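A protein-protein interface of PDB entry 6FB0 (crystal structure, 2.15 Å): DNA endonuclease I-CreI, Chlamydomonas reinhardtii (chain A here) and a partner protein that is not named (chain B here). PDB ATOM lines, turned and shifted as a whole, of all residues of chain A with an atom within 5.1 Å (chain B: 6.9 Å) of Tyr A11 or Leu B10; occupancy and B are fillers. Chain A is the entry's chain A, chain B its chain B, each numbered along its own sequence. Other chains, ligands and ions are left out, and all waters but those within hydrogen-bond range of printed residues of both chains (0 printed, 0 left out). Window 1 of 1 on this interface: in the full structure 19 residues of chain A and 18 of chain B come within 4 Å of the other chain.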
ATOM      1  N   GLU A   7     -12.948  12.894  30.621  1.00  0.00           N
ATOM      2  CA  GLU A   7     -14.135  13.606  30.177  1.00  0.00           C
ATOM      3  C   GLU A   7     -13.948  14.121  28.745  1.00  0.00           C
ATOM      4  O   GLU A   7     -14.897  14.171  27.966  1.00  0.00           O
ATOM      5  CB  GLU A   7     -14.501  14.747  31.133  1.00  0.00           C
ATOM      6  CG  GLU A   7     -14.956  14.271  32.514  1.00  0.00           C
ATOM      7  CD  GLU A   7     -15.724  15.345  33.287  1.00  0.00           C
ATOM      8  OE1 GLU A   7     -15.762  16.509  32.832  1.00  0.00           O
ATOM      9  OE2 GLU A   7     -16.299  15.020  34.350  1.00  0.00           O
ATOM     10  N   PHE A   8     -12.719  14.503  28.411  1.00  0.00           N
ATOM     11  CA  PHE A   8     -12.398  14.922  27.051  1.00  0.00           C
ATOM     12  C   PHE A   8     -12.635  13.757  26.090  1.00  0.00           C
ATOM     13  O   PHE A   8     -13.227  13.932  25.021  1.00  0.00           O
ATOM     14  CB  PHE A   8     -10.950  15.433  26.970  1.00  0.00           C
ATOM     15  CG  PHE A   8     -10.384  15.472  25.565  1.00  0.00           C
ATOM     16  CD1 PHE A   8     -10.730  16.493  24.687  1.00  0.00           C
ATOM     17  CD2 PHE A   8      -9.478  14.505  25.139  1.00  0.00           C
ATOM     18  CE1 PHE A   8     -10.193  16.544  23.393  1.00  0.00           C
ATOM     19  CE2 PHE A   8      -8.931  14.546  23.856  1.00  0.00           C
ATOM     20  CZ  PHE A   8      -9.296  15.566  22.976  1.00  0.00           C
ATOM     21  N   LEU A   9     -12.210  12.563  26.496  1.00  0.00           N
ATOM     22  CA  LEU A   9     -12.321  11.368  25.653  1.00  0.00           C
ATOM     23  C   LEU A   9     -13.757  10.910  25.403  1.00  0.00           C
ATOM     24  O   LEU A   9     -14.071  10.446  24.296  1.00  0.00           O
ATOM     25  CB  LEU A   9     -11.485  10.206  26.224  1.00  0.00           C
ATOM     26  CG  LEU A   9      -9.953  10.375  26.157  1.00  0.00           C
ATOM     27  CD1 LEU A   9      -9.258   9.294  26.970  1.00  0.00           C
ATOM     28  CD2 LEU A   9      -9.446  10.379  24.703  1.00  0.00           C
ATOM     29  N   LEU A  10     -14.616  11.024  26.420  1.00  0.00           N
ATOM     30  CA  LEU A  10     -16.022  10.646  26.279  1.00  0.00           C
ATOM     31  C   LEU A  10     -16.743  11.575  25.304  1.00  0.00           C
ATOM     32  O   LEU A  10     -17.428  11.109  24.401  1.00  0.00           O
ATOM     33  CB  LEU A  10     -16.754  10.632  27.637  1.00  0.00           C
ATOM     34  CG  LEU A  10     -16.531   9.441  28.586  1.00  0.00           C
ATOM     35  CD1 LEU A  10     -16.790   9.841  30.032  1.00  0.00           C
ATOM     36  CD2 LEU A  10     -17.378   8.229  28.205  1.00  0.00           C
ATOM     37  N   TYR A  11     -16.611  12.885  25.490  1.00  0.00           N
ATOM     38  CA  TYR A  11     -17.186  13.827  24.526  1.00  0.00           C
ATOM     39  C   TYR A  11     -16.627  13.616  23.107  1.00  0.00           C
ATOM     40  O   TYR A  11     -17.384  13.607  22.118  1.00  0.00           O
ATOM     41  CB  TYR A  11     -16.958  15.283  24.961  1.00  0.00           C
ATOM     42  CG  TYR A  11     -17.428  16.269  23.931  1.00  0.00           C
ATOM     43  CD1 TYR A  11     -16.603  16.622  22.854  1.00  0.00           C
ATOM     44  CD2 TYR A  11     -18.702  16.834  24.001  1.00  0.00           C
ATOM     45  CE1 TYR A  11     -17.025  17.504  21.872  1.00  0.00           C
ATOM     46  CE2 TYR A  11     -19.139  17.741  23.016  1.00  0.00           C
ATOM     47  CZ  TYR A  11     -18.286  18.065  21.954  1.00  0.00           C
ATOM     48  OH  TYR A  11     -18.674  18.952  20.977  1.00  0.00           O
ATOM     49  N   LEU A  12     -15.306  13.444  23.007  1.00  0.00           N
ATOM     50  CA  LEU A  12     -14.643  13.291  21.699  1.00  0.00           C
ATOM     51  C   LEU A  12     -15.090  12.011  20.988  1.00  0.00           C
ATOM     52  O   LEU A  12     -15.280  11.992  19.771  1.00  0.00           O
ATOM     53  CB  LEU A  12     -13.109  13.300  21.835  1.00  0.00           C
ATOM     54  CG  LEU A  12     -12.356  13.215  20.495  1.00  0.00           C
ATOM     55  CD1 LEU A  12     -12.874  14.274  19.520  1.00  0.00           C
ATOM     56  CD2 LEU A  12     -10.833  13.340  20.682  1.00  0.00           C
ATOM     57  N   ALA A  13     -15.273  10.944  21.752  1.00  0.00           N
ATOM     58  CA  ALA A  13     -15.756   9.703  21.175  1.00  0.00           C
ATOM     59  C   ALA A  13     -17.141   9.907  20.569  1.00  0.00           C
ATOM     60  O   ALA A  13     -17.441   9.390  19.491  1.00  0.00           O
ATOM     61  CB  ALA A  13     -15.781   8.572  22.222  1.00  0.00           C
ATOM     62  N   GLY A  14     -17.996  10.654  21.255  1.00  0.00           N
ATOM     63  CA  GLY A  14     -19.326  10.902  20.713  1.00  0.00           C
ATOM     64  C   GLY A  14     -19.230  11.693  19.410  1.00  0.00           C
ATOM     65  O   GLY A  14     -19.987  11.478  18.459  1.00  0.00           O
ATOM     66  N   PHE A  15     -18.300  12.641  19.374  1.00  0.00           N
ATOM     67  CA  PHE A  15     -18.184  13.517  18.216  1.00  0.00           C
ATOM     68  C   PHE A  15     -17.564  12.763  17.034  1.00  0.00           C
ATOM     69  O   PHE A  15     -17.925  12.978  15.884  1.00  0.00           O
ATOM     70  CB  PHE A  15     -17.377  14.770  18.556  1.00  0.00           C
ATOM     71  CG  PHE A  15     -17.536  15.877  17.541  1.00  0.00           C
ATOM     72  CD1 PHE A  15     -18.612  16.746  17.614  1.00  0.00           C
ATOM     73  CD2 PHE A  15     -16.630  16.026  16.510  1.00  0.00           C
ATOM     74  CE1 PHE A  15     -18.771  17.757  16.680  1.00  0.00           C
ATOM     75  CE2 PHE A  15     -16.786  17.042  15.566  1.00  0.00           C
ATOM     76  CZ  PHE A  15     -17.849  17.903  15.658  1.00  0.00           C
ATOM     77  N   PHE A  53     -13.018  24.893  15.870  1.00  0.00           N
ATOM     78  CA  PHE A  53     -13.249  23.681  16.654  1.00  0.00           C
ATOM     79  C   PHE A  53     -12.180  22.620  16.342  1.00  0.00           C
ATOM     80  O   PHE A  53     -11.655  21.957  17.242  1.00  0.00           O
ATOM     81  CB  PHE A  53     -14.651  23.159  16.346  1.00  0.00           C
ATOM     82  CG  PHE A  53     -15.117  22.060  17.246  1.00  0.00           C
ATOM     83  CD1 PHE A  53     -14.972  20.734  16.873  1.00  0.00           C
ATOM     84  CD2 PHE A  53     -15.738  22.350  18.451  1.00  0.00           C
ATOM     85  CE1 PHE A  53     -15.433  19.711  17.697  1.00  0.00           C
ATOM     86  CE2 PHE A  53     -16.197  21.334  19.274  1.00  0.00           C
ATOM     87  CZ  PHE A  53     -16.045  20.018  18.897  1.00  0.00           C
ATOM     88  N   ASN B   5     -27.063   9.855  33.853  1.00  0.00           N
ATOM     89  CA  ASN B   5     -25.648   9.695  34.207  1.00  0.00           C
ATOM     90  C   ASN B   5     -24.730  10.664  33.454  1.00  0.00           C
ATOM     91  O   ASN B   5     -24.949  10.966  32.276  1.00  0.00           O
ATOM     92  CB  ASN B   5     -25.175   8.261  33.938  1.00  0.00           C
ATOM     93  CG  ASN B   5     -25.752   7.260  34.902  1.00  0.00           C
ATOM     94  OD1 ASN B   5     -26.059   7.582  36.056  1.00  0.00           O
ATOM     95  ND2 ASN B   5     -25.893   6.025  34.442  1.00  0.00           N
ATOM     96  N   LYS B   6     -23.679  11.120  34.123  1.00  0.00           N
ATOM     97  CA  LYS B   6     -22.785  12.116  33.538  1.00  0.00           C
ATOM     98  C   LYS B   6     -21.993  11.591  32.337  1.00  0.00           C
ATOM     99  O   LYS B   6     -21.804  12.289  31.346  1.00  0.00           O
ATOM    100  CB  LYS B   6     -21.813  12.629  34.592  1.00  0.00           C
ATOM    101  CG  LYS B   6     -20.912  13.749  34.100  1.00  0.00           C
ATOM    102  CD  LYS B   6     -20.066  14.282  35.240  1.00  0.00           C
ATOM    103  CE  LYS B   6     -19.267  15.494  34.820  1.00  0.00           C
ATOM    104  NZ  LYS B   6     -18.588  16.044  36.009  1.00  0.00           N
ATOM    105  N   GLU B   7     -21.509  10.363  32.429  1.00  0.00           N
ATOM    106  CA  GLU B   7     -20.694   9.840  31.351  1.00  0.00           C
ATOM    107  C   GLU B   7     -21.546   9.665  30.110  1.00  0.00           C
ATOM    108  O   GLU B   7     -21.059   9.811  28.985  1.00  0.00           O
ATOM    109  CB  GLU B   7     -19.984   8.552  31.768  1.00  0.00           C
ATOM    110  CG  GLU B   7     -18.951   8.809  32.866  1.00  0.00           C
ATOM    111  CD  GLU B   7     -18.054   7.615  33.149  1.00  0.00           C
ATOM    112  OE1 GLU B   7     -18.443   6.474  32.829  1.00  0.00           O
ATOM    113  OE2 GLU B   7     -16.953   7.823  33.696  1.00  0.00           O
ATOM    114  N   PHE B   8     -22.827   9.385  30.336  1.00  0.00           N
ATOM    115  CA  PHE B   8     -23.815   9.296  29.272  1.00  0.00           C
ATOM    116  C   PHE B   8     -24.031  10.656  28.606  1.00  0.00           C
ATOM    117  O   PHE B   8     -23.938  10.761  27.385  1.00  0.00           O
ATOM    118  CB  PHE B   8     -25.125   8.710  29.811  1.00  0.00           C
ATOM    119  CG  PHE B   8     -26.315   8.907  28.900  1.00  0.00           C
ATOM    120  CD1 PHE B   8     -26.513   8.078  27.801  1.00  0.00           C
ATOM    121  CD2 PHE B   8     -27.249   9.903  29.161  1.00  0.00           C
ATOM    122  CE1 PHE B   8     -27.617   8.249  26.975  1.00  0.00           C
ATOM    123  CE2 PHE B   8     -28.348  10.081  28.336  1.00  0.00           C
ATOM    124  CZ  PHE B   8     -28.533   9.252  27.244  1.00  0.00           C
ATOM    125  N   LEU B   9     -24.294  11.695  29.401  1.00  0.00           N
ATOM    126  CA  LEU B   9     -24.451  13.067  28.873  1.00  0.00           C
ATOM    127  C   LEU B   9     -23.224  13.588  28.090  1.00  0.00           C
ATOM    128  O   LEU B   9     -23.370  14.297  27.092  1.00  0.00           O
ATOM    129  CB  LEU B   9     -24.805  14.052  29.998  1.00  0.00           C
ATOM    130  CG  LEU B   9     -26.164  13.769  30.678  1.00  0.00           C
ATOM    131  CD1 LEU B   9     -26.362  14.546  32.014  1.00  0.00           C
ATOM    132  CD2 LEU B   9     -27.294  14.038  29.692  1.00  0.00           C
ATOM    133  N   LEU B  10     -22.028  13.235  28.556  1.00  0.00           N
ATOM    134  CA  LEU B  10     -20.778  13.648  27.919  1.00  0.00           C
ATOM    135  C   LEU B  10     -20.623  13.068  26.516  1.00  0.00           C
ATOM    136  O   LEU B  10     -20.286  13.779  25.566  1.00  0.00           O
ATOM    137  CB  LEU B  10     -19.579  13.228  28.775  1.00  0.00           C
ATOM    138  CG  LEU B  10     -19.181  14.169  29.920  1.00  0.00           C
ATOM    139  CD1 LEU B  10     -18.406  13.436  31.016  1.00  0.00           C
ATOM    140  CD2 LEU B  10     -18.388  15.354  29.382  1.00  0.00           C
ATOM    141  N   TYR B  11     -20.855  11.766  26.390  1.00  0.00           N
ATOM    142  CA  TYR B  11     -20.760  11.117  25.097  1.00  0.00           C
ATOM    143  C   TYR B  11     -21.876  11.624  24.187  1.00  0.00           C
ATOM    144  O   TYR B  11     -21.637  11.930  23.021  1.00  0.00           O
ATOM    145  CB  TYR B  11     -20.841   9.593  25.237  1.00  0.00           C
ATOM    146  CG  TYR B  11     -20.955   8.907  23.905  1.00  0.00           C
ATOM    147  CD1 TYR B  11     -22.194   8.760  23.299  1.00  0.00           C
ATOM    148  CD2 TYR B  11     -19.818   8.445  23.223  1.00  0.00           C
ATOM    149  CE1 TYR B  11     -22.322   8.151  22.064  1.00  0.00           C
ATOM    150  CE2 TYR B  11     -19.936   7.832  21.979  1.00  0.00           C
ATOM    151  CZ  TYR B  11     -21.198   7.692  21.407  1.00  0.00           C
ATOM    152  OH  TYR B  11     -21.367   7.088  20.183  1.00  0.00           O
ATOM    153  N   LEU B  12     -23.092  11.726  24.723  1.00  0.00           N
ATOM    154  CA  LEU B  12     -24.248  12.098  23.902  1.00  0.00           C
ATOM    155  C   LEU B  12     -24.089  13.525  23.354  1.00  0.00           C
ATOM    156  O   LEU B  12     -24.383  13.786  22.190  1.00  0.00           O
ATOM    157  CB  LEU B  12     -25.561  11.959  24.696  1.00  0.00           C
ATOM    158  CG  LEU B  12     -26.842  12.213  23.891  1.00  0.00           C
ATOM    159  CD1 LEU B  12     -26.893  11.288  22.654  1.00  0.00           C
ATOM    160  CD2 LEU B  12     -28.105  12.055  24.755  1.00  0.00           C
ATOM    161  N   ALA B  13     -23.629  14.440  24.212  1.00  0.00           N
ATOM    162  CA  ALA B  13     -23.341  15.807  23.796  1.00  0.00           C
ATOM    163  C   ALA B  13     -22.404  15.827  22.578  1.00  0.00           C
ATOM    164  O   ALA B  13     -22.678  16.502  21.595  1.00  0.00           O
ATOM    165  CB  ALA B  13     -22.748  16.604  24.940  1.00  0.00           C
ATOM    166  N   GLY B  14     -21.309  15.077  22.641  1.00  0.00           N
ATOM    167  CA  GLY B  14     -20.437  14.939  21.487  1.00  0.00           C
ATOM    168  C   GLY B  14     -21.171  14.430  20.249  1.00  0.00           C
ATOM    169  O   GLY B  14     -20.998  14.949  19.133  1.00  0.00           O
ATOM    170  N   PHE B  15     -21.984  13.397  20.431  1.00  0.00           N
ATOM    171  CA  PHE B  15     -22.702  12.820  19.310  1.00  0.00           C
ATOM    172  C   PHE B  15     -23.762  13.789  18.763  1.00  0.00           C
ATOM    173  O   PHE B  15     -24.022  13.835  17.561  1.00  0.00           O
ATOM    174  CB  PHE B  15     -23.340  11.476  19.684  1.00  0.00           C
ATOM    175  CG  PHE B  15     -23.736  10.651  18.490  1.00  0.00           C
ATOM    176  CD1 PHE B  15     -22.855   9.732  17.947  1.00  0.00           C
ATOM    177  CD2 PHE B  15     -24.980  10.818  17.895  1.00  0.00           C
ATOM    178  CE1 PHE B  15     -23.214   8.978  16.837  1.00  0.00           C
ATOM    179  CE2 PHE B  15     -25.348  10.060  16.780  1.00  0.00           C
ATOM    180  CZ  PHE B  15     -24.468   9.145  16.251  1.00  0.00           C
ATOM    181  N   ASP B  17     -23.652  17.253  19.039  1.00  0.00           N
ATOM    182  CA  ASP B  17     -22.891  18.286  18.342  1.00  0.00           C
ATOM    183  C   ASP B  17     -22.492  17.795  16.945  1.00  0.00           C
ATOM    184  O   ASP B  17     -22.337  18.587  16.016  1.00  0.00           O
ATOM    185  CB  ASP B  17     -21.639  18.670  19.137  1.00  0.00           C
ATOM    186  CG  ASP B  17     -21.897  19.762  20.164  1.00  0.00           C
ATOM    187  OD1 ASP B  17     -22.939  20.450  20.101  1.00  0.00           O
ATOM    188  OD2 ASP B  17     -21.037  19.937  21.042  1.00  0.00           O
ATOM    189  N   GLY B  18     -22.332  16.486  16.802  1.00  0.00           N
ATOM    190  CA  GLY B  18     -21.969  15.898  15.521  1.00  0.00           C
ATOM    191  C   GLY B  18     -23.162  15.598  14.617  1.00  0.00           C
ATOM    192  O   GLY B  18     -23.328  16.240  13.595  1.00  0.00           O
ATOM    193  N   LEU B  90     -28.120  18.300  29.437  1.00  0.00           N
ATOM    194  CA  LEU B  90     -27.180  18.113  28.334  1.00  0.00           C
ATOM    195  C   LEU B  90     -26.375  19.380  28.079  1.00  0.00           C
ATOM    196  O   LEU B  90     -25.188  19.345  27.746  1.00  0.00           O
ATOM    197  CB  LEU B  90     -27.948  17.788  27.061  1.00  0.00           C
ATOM    198  CG  LEU B  90     -27.127  17.294  25.881  1.00  0.00           C
ATOM    199  CD1 LEU B  90     -26.522  15.935  26.202  1.00  0.00           C
ATOM    200  CD2 LEU B  90     -27.993  17.229  24.620  1.00  0.00           C
ATOM    201  N   PHE B  93     -22.648  20.308  28.582  1.00  0.00           N
ATOM    202  CA  PHE B  93     -21.607  19.550  27.898  1.00  0.00           C
ATOM    203  C   PHE B  93     -21.543  19.832  26.389  1.00  0.00           C
ATOM    204  O   PHE B  93     -20.611  19.407  25.698  1.00  0.00           O
ATOM    205  CB  PHE B  93     -21.799  18.053  28.184  1.00  0.00           C
ATOM    206  CG  PHE B  93     -21.919  17.741  29.659  1.00  0.00           C
ATOM    207  CD1 PHE B  93     -20.810  17.815  30.484  1.00  0.00           C
ATOM    208  CD2 PHE B  93     -23.143  17.416  30.219  1.00  0.00           C
ATOM    209  CE1 PHE B  93     -20.915  17.552  31.844  1.00  0.00           C
ATOM    210  CE2 PHE B  93     -23.252  17.135  31.586  1.00  0.00           C
ATOM    211  CZ  PHE B  93     -22.138  17.203  32.391  1.00  0.00           C
ATOM    212  N   LEU B  94     -22.532  20.556  25.883  1.00  0.00           N
ATOM    213  CA  LEU B  94     -22.560  20.897  24.465  1.00  0.00           C
ATOM    214  C   LEU B  94     -21.452  21.886  24.125  1.00  0.00           C
ATOM    215  O   LEU B  94     -21.110  22.746  24.934  1.00  0.00           O
ATOM    216  CB  LEU B  94     -23.918  21.487  24.090  1.00  0.00           C
ATOM    217  CG  LEU B  94     -25.065  20.479  24.058  1.00  0.00           C
ATOM    218  CD1 LEU B  94     -26.410  21.187  23.883  1.00  0.00           C
ATOM    219  CD2 LEU B  94     -24.793  19.458  22.939  1.00  0.00           C
ATOM    220  N   LYS B  95     -20.903  21.766  22.920  1.00  0.00           N
ATOM    221  CA  LYS B  95     -19.869  22.698  22.466  1.00  0.00           C
ATOM    222  C   LYS B  95     -20.321  23.500  21.250  1.00  0.00           C
ATOM    223  O   LYS B  95     -20.169  24.716  21.217  1.00  0.00           O
ATOM    224  CB  LYS B  95     -18.559  21.960  22.164  1.00  0.00           C
ATOM    225  CG  LYS B  95     -17.839  21.444  23.406  1.00  0.00           C
ATOM    226  CD  LYS B  95     -16.473  20.877  23.049  1.00  0.00           C
ATOM    227  CE  LYS B  95     -15.618  20.617  24.285  1.00  0.00           C
ATOM    228  NZ  LYS B  95     -16.117  19.465  25.073  1.00  0.00           N
ATOM    229  N   LEU B  96     -20.884  22.826  20.251  1.00  0.00           N
ATOM    230  CA  LEU B  96     -21.307  23.528  19.041  1.00  0.00           C
ATOM    231  C   LEU B  96     -22.750  24.019  19.115  1.00  0.00           C
ATOM    232  O   LEU B  96     -23.108  24.986  18.438  1.00  0.00           O
ATOM    233  CB  LEU B  96     -21.133  22.649  17.805  1.00  0.00           C
ATOM    234  CG  LEU B  96     -19.719  22.215  17.420  1.00  0.00           C
ATOM    235  CD1 LEU B  96     -19.762  21.406  16.114  1.00  0.00           C
ATOM    236  CD2 LEU B  96     -18.805  23.434  17.295  1.00  0.00           C
ATOM    237  N   LYS B  97     -23.570  23.365  19.939  1.00  0.00           N
ATOM    238  CA  LYS B  97     -25.006  23.645  19.953  1.00  0.00           C
ATOM    239  C   LYS B  97     -25.495  24.134  21.308  1.00  0.00           C
ATOM    240  O   LYS B  97     -26.689  24.132  21.586  1.00  0.00           O
ATOM    241  CB  LYS B  97     -25.808  22.409  19.503  1.00  0.00           C
ATOM    242  CG  LYS B  97     -25.469  21.949  18.091  1.00  0.00           C
ATOM    243  CD  LYS B  97     -26.137  20.627  17.722  1.00  0.00           C
ATOM    244  CE  LYS B  97     -25.622  20.074  16.394  1.00  0.00           C
ATOM    245  NZ  LYS B  97     -26.333  20.666  15.218  1.00  0.00           N
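OE2 of Glu A7 lies within salt-bridge range of NZ of Lys B6 (3.0 Å). The side-chain carboxylate (OD2) of Asp B17 lies within hydrogen-bond range of the side-chain hydroxyl (OH) of Tyr A11, 2.6 Å away. N of Phe B15 sits close to O of Gly A14.
OD2 of Asp B17 lies within hydrogen-bond range of N of Lys B95 (2.6 Å). N of Leu B96 sits at hydrogen-bond distance from OD2 of Asp B17 (3.0 Å). The backbone NH of Lys B97 sits at hydrogen-bond distance from the side-chain carboxylate of Asp B17 (3.0 Å).
Among the printed residues, pairs that only touch across the chains: Glu A7 with Leu B10, Leu A10 with Glu B7, Leu A10 with Tyr B11, Tyr A11 with Leu B10, Tyr A11 with Ala B13, Tyr A11 with Gly B14, Tyr A11 with Phe B93, Tyr A11 with Lys B95, Ala A13 with Tyr B11, Gly A14 with Tyr B11, Gly A14 with Gly B14, Phe A15 with Gly B14, Phe A15 with Phe B15, Phe A15 with Asp B17, Phe A15 with Gly B18, Phe A15 with Leu B96, Phe A53 with Lys B95 and Phe A53 with Leu B96.
Tyr A11 touches just these residues of chain B: Leu B10 (3.3 Å), Ala B13 (3.8 Å), Gly B14 (3.4 Å), Asp B17 (2.6 Å), Phe B93 (3.5 Å) and Lys B95 (3.2 Å). Printed residues of chain A within 4 Å of Leu B10: Glu A7 and Tyr A11. Of the printed residues of chain B, Ala A13 touches Tyr B11. Of the printed residues of chain B, Phe A53 touches Lys B95 and Leu B96.
Of the 10 printed residues of chain A, 7 touch a printed residue of chain B. Among the printed residues, 21 pairs touch across the chains.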
